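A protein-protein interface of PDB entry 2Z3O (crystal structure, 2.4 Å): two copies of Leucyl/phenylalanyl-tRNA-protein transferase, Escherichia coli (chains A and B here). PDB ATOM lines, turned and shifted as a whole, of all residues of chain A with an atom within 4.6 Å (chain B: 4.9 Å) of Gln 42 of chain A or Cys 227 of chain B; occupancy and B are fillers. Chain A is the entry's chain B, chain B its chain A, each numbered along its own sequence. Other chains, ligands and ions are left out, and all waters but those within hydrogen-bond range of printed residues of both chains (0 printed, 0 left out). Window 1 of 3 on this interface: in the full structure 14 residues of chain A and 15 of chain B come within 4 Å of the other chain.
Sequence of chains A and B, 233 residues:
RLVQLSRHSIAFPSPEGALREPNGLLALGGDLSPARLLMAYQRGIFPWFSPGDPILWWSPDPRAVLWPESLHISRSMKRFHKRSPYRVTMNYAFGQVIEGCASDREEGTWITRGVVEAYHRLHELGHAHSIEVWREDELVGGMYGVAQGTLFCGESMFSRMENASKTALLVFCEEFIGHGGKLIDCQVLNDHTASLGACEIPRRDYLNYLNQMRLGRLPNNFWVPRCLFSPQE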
ATOM      1  N   LEU A  38     -20.879  -4.632 -15.391  1.00  0.00           N
ATOM      2  CA  LEU A  38     -20.280  -5.842 -14.845  1.00  0.00           C
ATOM      3  C   LEU A  38     -20.737  -7.060 -15.636  1.00  0.00           C
ATOM      4  O   LEU A  38     -19.949  -7.970 -15.893  1.00  0.00           O
ATOM      5  CB  LEU A  38     -20.650  -5.994 -13.375  1.00  0.00           C
ATOM      6  CG  LEU A  38     -19.542  -5.671 -12.374  1.00  0.00           C
ATOM      7  CD1 LEU A  38     -18.479  -4.796 -13.011  1.00  0.00           C
ATOM      8  CD2 LEU A  38     -20.163  -4.993 -11.165  1.00  0.00           C
ATOM      9  N   MET A  39     -22.011  -7.072 -16.026  1.00  0.00           N
ATOM     10  CA  MET A  39     -22.543  -8.179 -16.812  1.00  0.00           C
ATOM     11  C   MET A  39     -21.851  -8.209 -18.178  1.00  0.00           C
ATOM     12  O   MET A  39     -21.514  -9.275 -18.704  1.00  0.00           O
ATOM     13  CB  MET A  39     -24.052  -8.028 -16.988  1.00  0.00           C
ATOM     14  CG  MET A  39     -24.868  -8.381 -15.743  1.00  0.00           C
ATOM     15  SD  MET A  39     -24.883 -10.167 -15.383  1.00  0.00           S
ATOM     16  CE  MET A  39     -24.333 -10.210 -13.707  1.00  0.00           C
ATOM     17  N   ALA A  40     -21.625  -7.027 -18.742  1.00  0.00           N
ATOM     18  CA  ALA A  40     -20.977  -6.918 -20.043  1.00  0.00           C
ATOM     19  C   ALA A  40     -19.528  -7.399 -20.020  1.00  0.00           C
ATOM     20  O   ALA A  40     -19.160  -8.270 -20.805  1.00  0.00           O
ATOM     21  CB  ALA A  40     -21.036  -5.486 -20.538  1.00  0.00           C
ATOM     22  N   TYR A  41     -18.716  -6.833 -19.126  1.00  0.00           N
ATOM     23  CA  TYR A  41     -17.304  -7.205 -19.035  1.00  0.00           C
ATOM     24  C   TYR A  41     -17.151  -8.671 -18.705  1.00  0.00           C
ATOM     25  O   TYR A  41     -16.164  -9.311 -19.064  1.00  0.00           O
ATOM     26  CB  TYR A  41     -16.601  -6.353 -17.986  1.00  0.00           C
ATOM     27  CG  TYR A  41     -16.246  -4.974 -18.504  1.00  0.00           C
ATOM     28  CD1 TYR A  41     -15.071  -4.759 -19.220  1.00  0.00           C
ATOM     29  CD2 TYR A  41     -17.113  -3.894 -18.316  1.00  0.00           C
ATOM     30  CE1 TYR A  41     -14.769  -3.508 -19.735  1.00  0.00           C
ATOM     31  CE2 TYR A  41     -16.820  -2.634 -18.833  1.00  0.00           C
ATOM     32  CZ  TYR A  41     -15.649  -2.446 -19.538  1.00  0.00           C
ATOM     33  OH  TYR A  41     -15.359  -1.195 -20.045  1.00  0.00           O
ATOM     34  N   GLN A  42     -18.163  -9.196 -18.034  1.00  0.00           N
ATOM     35  CA  GLN A  42     -18.201 -10.588 -17.632  1.00  0.00           C
ATOM     36  C   GLN A  42     -18.396 -11.484 -18.846  1.00  0.00           C
ATOM     37  O   GLN A  42     -18.061 -12.668 -18.814  1.00  0.00           O
ATOM     38  CB  GLN A  42     -19.357 -10.786 -16.658  1.00  0.00           C
ATOM     39  CG  GLN A  42     -19.426 -12.132 -15.988  1.00  0.00           C
ATOM     40  CD  GLN A  42     -20.551 -12.182 -14.982  1.00  0.00           C
ATOM     41  OE1 GLN A  42     -20.644 -13.105 -14.166  1.00  0.00           O
ATOM     42  NE2 GLN A  42     -21.425 -11.182 -15.038  1.00  0.00           N
ATOM     43  N   ARG A  43     -18.934 -10.913 -19.920  1.00  0.00           N
ATOM     44  CA  ARG A  43     -19.184 -11.679 -21.134  1.00  0.00           C
ATOM     45  C   ARG A  43     -18.326 -11.250 -22.309  1.00  0.00           C
ATOM     46  O   ARG A  43     -18.618 -11.608 -23.444  1.00  0.00           O
ATOM     47  CB  ARG A  43     -20.656 -11.567 -21.533  1.00  0.00           C
ATOM     48  CG  ARG A  43     -21.613 -12.011 -20.453  1.00  0.00           C
ATOM     49  CD  ARG A  43     -22.409 -13.214 -20.906  1.00  0.00           C
ATOM     50  NE  ARG A  43     -23.422 -12.863 -21.892  1.00  0.00           N
ATOM     51  CZ  ARG A  43     -23.801 -13.668 -22.876  1.00  0.00           C
ATOM     52  NH1 ARG A  43     -23.242 -14.865 -22.999  1.00  0.00           N
ATOM     53  NH2 ARG A  43     -24.739 -13.284 -23.736  1.00  0.00           N
ATOM     54  N   GLY A  44     -17.282 -10.470 -22.049  1.00  0.00           N
ATOM     55  CA  GLY A  44     -16.409 -10.027 -23.127  1.00  0.00           C
ATOM     56  C   GLY A  44     -17.010  -8.940 -23.993  1.00  0.00           C
ATOM     57  O   GLY A  44     -16.735  -8.850 -25.196  1.00  0.00           O
ATOM     58  N   GLN A 148     -11.107  -8.228 -14.057  1.00  0.00           N
ATOM     59  CA  GLN A 148     -11.947  -9.376 -14.296  1.00  0.00           C
ATOM     60  C   GLN A 148     -11.096 -10.550 -13.806  1.00  0.00           C
ATOM     61  O   GLN A 148     -10.503 -11.287 -14.594  1.00  0.00           O
ATOM     62  CB  GLN A 148     -12.213  -9.461 -15.797  1.00  0.00           C
ATOM     63  CG  GLN A 148     -13.526 -10.076 -16.217  1.00  0.00           C
ATOM     64  CD  GLN A 148     -14.731  -9.319 -15.714  1.00  0.00           C
ATOM     65  OE1 GLN A 148     -14.618  -8.213 -15.184  1.00  0.00           O
ATOM     66  NE2 GLN A 148     -15.903  -9.911 -15.891  1.00  0.00           N
ATOM     67  N   LEU A 210     -11.283 -15.445 -20.928  1.00  0.00           N
ATOM     68  CA  LEU A 210     -12.058 -14.590 -20.037  1.00  0.00           C
ATOM     69  C   LEU A 210     -12.776 -15.289 -18.888  1.00  0.00           C
ATOM     70  O   LEU A 210     -12.527 -14.965 -17.736  1.00  0.00           O
ATOM     71  CB  LEU A 210     -13.049 -13.742 -20.855  1.00  0.00           C
ATOM     72  CG  LEU A 210     -14.005 -12.745 -20.176  1.00  0.00           C
ATOM     73  CD1 LEU A 210     -15.256 -13.459 -19.758  1.00  0.00           C
ATOM     74  CD2 LEU A 210     -13.344 -12.087 -18.979  1.00  0.00           C
ATOM     75  N   ARG A 214     -11.776 -14.817 -14.944  1.00  0.00           N
ATOM     76  CA  ARG A 214     -12.674 -14.030 -14.090  1.00  0.00           C
ATOM     77  C   ARG A 214     -12.929 -14.669 -12.729  1.00  0.00           C
ATOM     78  O   ARG A 214     -13.198 -13.969 -11.761  1.00  0.00           O
ATOM     79  CB  ARG A 214     -14.015 -13.748 -14.786  1.00  0.00           C
ATOM     80  CG  ARG A 214     -14.656 -14.920 -15.482  1.00  0.00           C
ATOM     81  CD  ARG A 214     -15.834 -14.452 -16.343  1.00  0.00           C
ATOM     82  NE  ARG A 214     -17.055 -14.296 -15.563  1.00  0.00           N
ATOM     83  CZ  ARG A 214     -17.852 -15.304 -15.225  1.00  0.00           C
ATOM     84  NH1 ARG A 214     -17.565 -16.541 -15.604  1.00  0.00           N
ATOM     85  NH2 ARG A 214     -18.927 -15.078 -14.492  1.00  0.00           N
ATOM     86  N   ARG B  87     -32.089 -11.508  -9.994  1.00  0.00           N
ATOM     87  CA  ARG B  87     -30.753 -11.968 -10.327  1.00  0.00           C
ATOM     88  C   ARG B  87     -29.957 -11.831  -9.021  1.00  0.00           C
ATOM     89  O   ARG B  87     -30.162 -10.897  -8.259  1.00  0.00           O
ATOM     90  CB  ARG B  87     -30.172 -11.091 -11.444  1.00  0.00           C
ATOM     91  CG  ARG B  87     -28.824 -11.532 -11.978  1.00  0.00           C
ATOM     92  CD  ARG B  87     -28.459 -10.790 -13.281  1.00  0.00           C
ATOM     93  NE  ARG B  87     -28.930 -11.480 -14.488  1.00  0.00           N
ATOM     94  CZ  ARG B  87     -29.920 -11.060 -15.279  1.00  0.00           C
ATOM     95  NH1 ARG B  87     -30.578  -9.934 -15.005  1.00  0.00           N
ATOM     96  NH2 ARG B  87     -30.245 -11.759 -16.364  1.00  0.00           N
ATOM     97  N   VAL B  88     -29.087 -12.783  -8.729  1.00  0.00           N
ATOM     98  CA  VAL B  88     -28.285 -12.664  -7.524  1.00  0.00           C
ATOM     99  C   VAL B  88     -26.795 -12.704  -7.865  1.00  0.00           C
ATOM    100  O   VAL B  88     -26.344 -13.576  -8.601  1.00  0.00           O
ATOM    101  CB  VAL B  88     -28.590 -13.784  -6.499  1.00  0.00           C
ATOM    102  CG1 VAL B  88     -27.755 -13.561  -5.235  1.00  0.00           C
ATOM    103  CG2 VAL B  88     -30.077 -13.806  -6.160  1.00  0.00           C
ATOM    104  N   THR B  89     -26.040 -11.748  -7.339  1.00  0.00           N
ATOM    105  CA  THR B  89     -24.597 -11.699  -7.574  1.00  0.00           C
ATOM    106  C   THR B  89     -23.900 -11.597  -6.230  1.00  0.00           C
ATOM    107  O   THR B  89     -24.538 -11.326  -5.221  1.00  0.00           O
ATOM    108  CB  THR B  89     -24.178 -10.473  -8.424  1.00  0.00           C
ATOM    109  OG1 THR B  89     -24.534  -9.263  -7.739  1.00  0.00           O
ATOM    110  CG2 THR B  89     -24.867 -10.503  -9.788  1.00  0.00           C
ATOM    111  N   TYR B  92     -20.624  -7.606  -6.001  1.00  0.00           N
ATOM    112  CA  TYR B  92     -20.737  -6.737  -7.154  1.00  0.00           C
ATOM    113  C   TYR B  92     -20.809  -5.308  -6.645  1.00  0.00           C
ATOM    114  O   TYR B  92     -20.179  -4.421  -7.197  1.00  0.00           O
ATOM    115  CB  TYR B  92     -22.033  -7.030  -7.890  1.00  0.00           C
ATOM    116  CG  TYR B  92     -21.907  -7.827  -9.154  1.00  0.00           C
ATOM    117  CD1 TYR B  92     -21.091  -8.951  -9.224  1.00  0.00           C
ATOM    118  CD2 TYR B  92     -22.666  -7.496 -10.266  1.00  0.00           C
ATOM    119  CE1 TYR B  92     -21.042  -9.720 -10.364  1.00  0.00           C
ATOM    120  CE2 TYR B  92     -22.621  -8.261 -11.412  1.00  0.00           C
ATOM    121  CZ  TYR B  92     -21.810  -9.368 -11.454  1.00  0.00           C
ATOM    122  OH  TYR B  92     -21.762 -10.114 -12.597  1.00  0.00           O
ATOM    123  N   PRO B 225     -15.927 -11.802  -7.073  1.00  0.00           N
ATOM    124  CA  PRO B 225     -17.145 -11.291  -7.711  1.00  0.00           C
ATOM    125  C   PRO B 225     -17.669 -12.200  -8.798  1.00  0.00           C
ATOM    126  O   PRO B 225     -16.921 -12.615  -9.679  1.00  0.00           O
ATOM    127  CB  PRO B 225     -16.708  -9.932  -8.255  1.00  0.00           C
ATOM    128  CG  PRO B 225     -15.212 -10.118  -8.464  1.00  0.00           C
ATOM    129  CD  PRO B 225     -14.815 -10.848  -7.214  1.00  0.00           C
ATOM    130  N   ARG B 226     -18.963 -12.505  -8.741  1.00  0.00           N
ATOM    131  CA  ARG B 226     -19.579 -13.377  -9.740  1.00  0.00           C
ATOM    132  C   ARG B 226     -21.101 -13.462  -9.602  1.00  0.00           C
ATOM    133  O   ARG B 226     -21.677 -13.069  -8.588  1.00  0.00           O
ATOM    134  CB  ARG B 226     -18.981 -14.782  -9.632  1.00  0.00           C
ATOM    135  CG  ARG B 226     -19.273 -15.494  -8.310  1.00  0.00           C
ATOM    136  CD  ARG B 226     -18.009 -16.127  -7.722  1.00  0.00           C
ATOM    137  NE  ARG B 226     -18.260 -16.830  -6.464  1.00  0.00           N
ATOM    138  CZ  ARG B 226     -18.971 -17.948  -6.376  1.00  0.00           C
ATOM    139  NH1 ARG B 226     -19.494 -18.488  -7.477  1.00  0.00           N
ATOM    140  NH2 ARG B 226     -19.165 -18.522  -5.199  1.00  0.00           N
ATOM    141  N   CYS B 227     -21.750 -13.972 -10.640  1.00  0.00           N
ATOM    142  CA  CYS B 227     -23.194 -14.141 -10.619  1.00  0.00           C
ATOM    143  C   CYS B 227     -23.457 -15.471  -9.910  1.00  0.00           C
ATOM    144  O   CYS B 227     -22.709 -16.420 -10.098  1.00  0.00           O
ATOM    145  CB  CYS B 227     -23.737 -14.189 -12.049  1.00  0.00           C
ATOM    146  SG  CYS B 227     -25.541 -14.139 -12.173  1.00  0.00           S
ATOM    147  N   LEU B 228     -24.500 -15.532  -9.085  1.00  0.00           N
ATOM    148  CA  LEU B 228     -24.836 -16.764  -8.362  1.00  0.00           C
ATOM    149  C   LEU B 228     -26.114 -17.379  -8.906  1.00  0.00           C
ATOM    150  O   LEU B 228     -26.258 -18.598  -8.973  1.00  0.00           O
ATOM    151  CB  LEU B 228     -25.018 -16.480  -6.870  1.00  0.00           C
ATOM    152  CG  LEU B 228     -23.765 -16.020  -6.112  1.00  0.00           C
ATOM    153  CD1 LEU B 228     -24.192 -15.444  -4.773  1.00  0.00           C
ATOM    154  CD2 LEU B 228     -22.777 -17.177  -5.921  1.00  0.00           C
ATOM    155  N   PHE B 229     -27.043 -16.517  -9.299  1.00  0.00           N
ATOM    156  CA  PHE B 229     -28.307 -16.974  -9.813  1.00  0.00           C
ATOM    157  C   PHE B 229     -28.851 -16.010 -10.841  1.00  0.00           C
ATOM    158  O   PHE B 229     -29.061 -14.833 -10.552  1.00  0.00           O
ATOM    159  CB  PHE B 229     -29.299 -17.144  -8.657  1.00  0.00           C
ATOM    160  CG  PHE B 229     -30.700 -17.476  -9.097  1.00  0.00           C
ATOM    161  CD1 PHE B 229     -31.618 -16.463  -9.358  1.00  0.00           C
ATOM    162  CD2 PHE B 229     -31.087 -18.803  -9.283  1.00  0.00           C
ATOM    163  CE1 PHE B 229     -32.908 -16.765  -9.797  1.00  0.00           C
ATOM    164  CE2 PHE B 229     -32.370 -19.119  -9.723  1.00  0.00           C
ATOM    165  CZ  PHE B 229     -33.288 -18.097  -9.983  1.00  0.00           C
ATOM    166  N   SER B 230     -29.073 -16.523 -12.048  1.00  0.00           N
ATOM    167  CA  SER B 230     -29.614 -15.732 -13.148  1.00  0.00           C
ATOM    168  C   SER B 230     -31.096 -16.031 -13.320  1.00  0.00           C
ATOM    169  O   SER B 230     -31.494 -17.192 -13.397  1.00  0.00           O
ATOM    170  CB  SER B 230     -28.883 -16.053 -14.450  1.00  0.00           C
ATOM    171  OG  SER B 230     -27.526 -15.652 -14.374  1.00  0.00           O
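Among the printed residues, merely in contact across the chains: Leu 38 of chain A with Tyr 92 of chain B, Met 39 of chain A with Thr 89 of chain B, Met 39 of chain A with Tyr 92 of chain B and Gln 42 of chain A with Cys 227 of chain B.
Hydrophobic or aromatic side chains of chain A within 4 Å of the printed part of chain B: Leu 38 and Met 39. Hydrophobic or aromatic side chains of chain B that line the printed part of chain A: Tyr 92.
OH of Tyr 92 of chain B sits at hydrogen-bond distance from NE2 of Gln 42 of chain A, at 2.7 Å.
Gln 42 of chain A touches two residues of chain B. Of chain A, only Gln 42 (3.8 Å) comes within 4 Å of Cys 227 of chain B. Printed residues of chain B within 4 Å of Leu 38 of chain A: Tyr 92 (3.6 Å). Printed residues of chain A within 4 Å of Tyr 92 of chain B: Leu 38, Met 39 and Gln 42. Arg 87 of chain B touches none of the printed residues of chain A. Phe 229 of chain B touches none of the printed residues of chain A. The nearest residue of chain B that does not touch Gln 42 of chain A is Arg 226 of chain B (4.6 Å).
The side-chain hydroxyl (OG) of Ser 230 of chain B is in hydrogen-bond range of the side-chain sulfur (SG) of Cys 227 of chain B, 3.3 Å away. The backbone NH (N) of Gln 42 of chain A sits close to the side-chain amide nitrogen (NE2) of Gln 148 of chain A. The side-chain amide oxygen (OE1) of Gln 42 of chain A lies within hydrogen-bond range of the guanidinium group (NH2) of Arg 214 of chain A. The side-chain sulfur (SD) of Met 39 of chain A sits close to the side-chain amide nitrogen (NE2) of Gln 42 of chain A, at 3.6 Å. The side-chain sulfur (SG) of Cys 227 of chain B sits close to the backbone carbonyl oxygen (O) of Val 88 of chain B (3.7 Å).
No position is printed for both chains.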
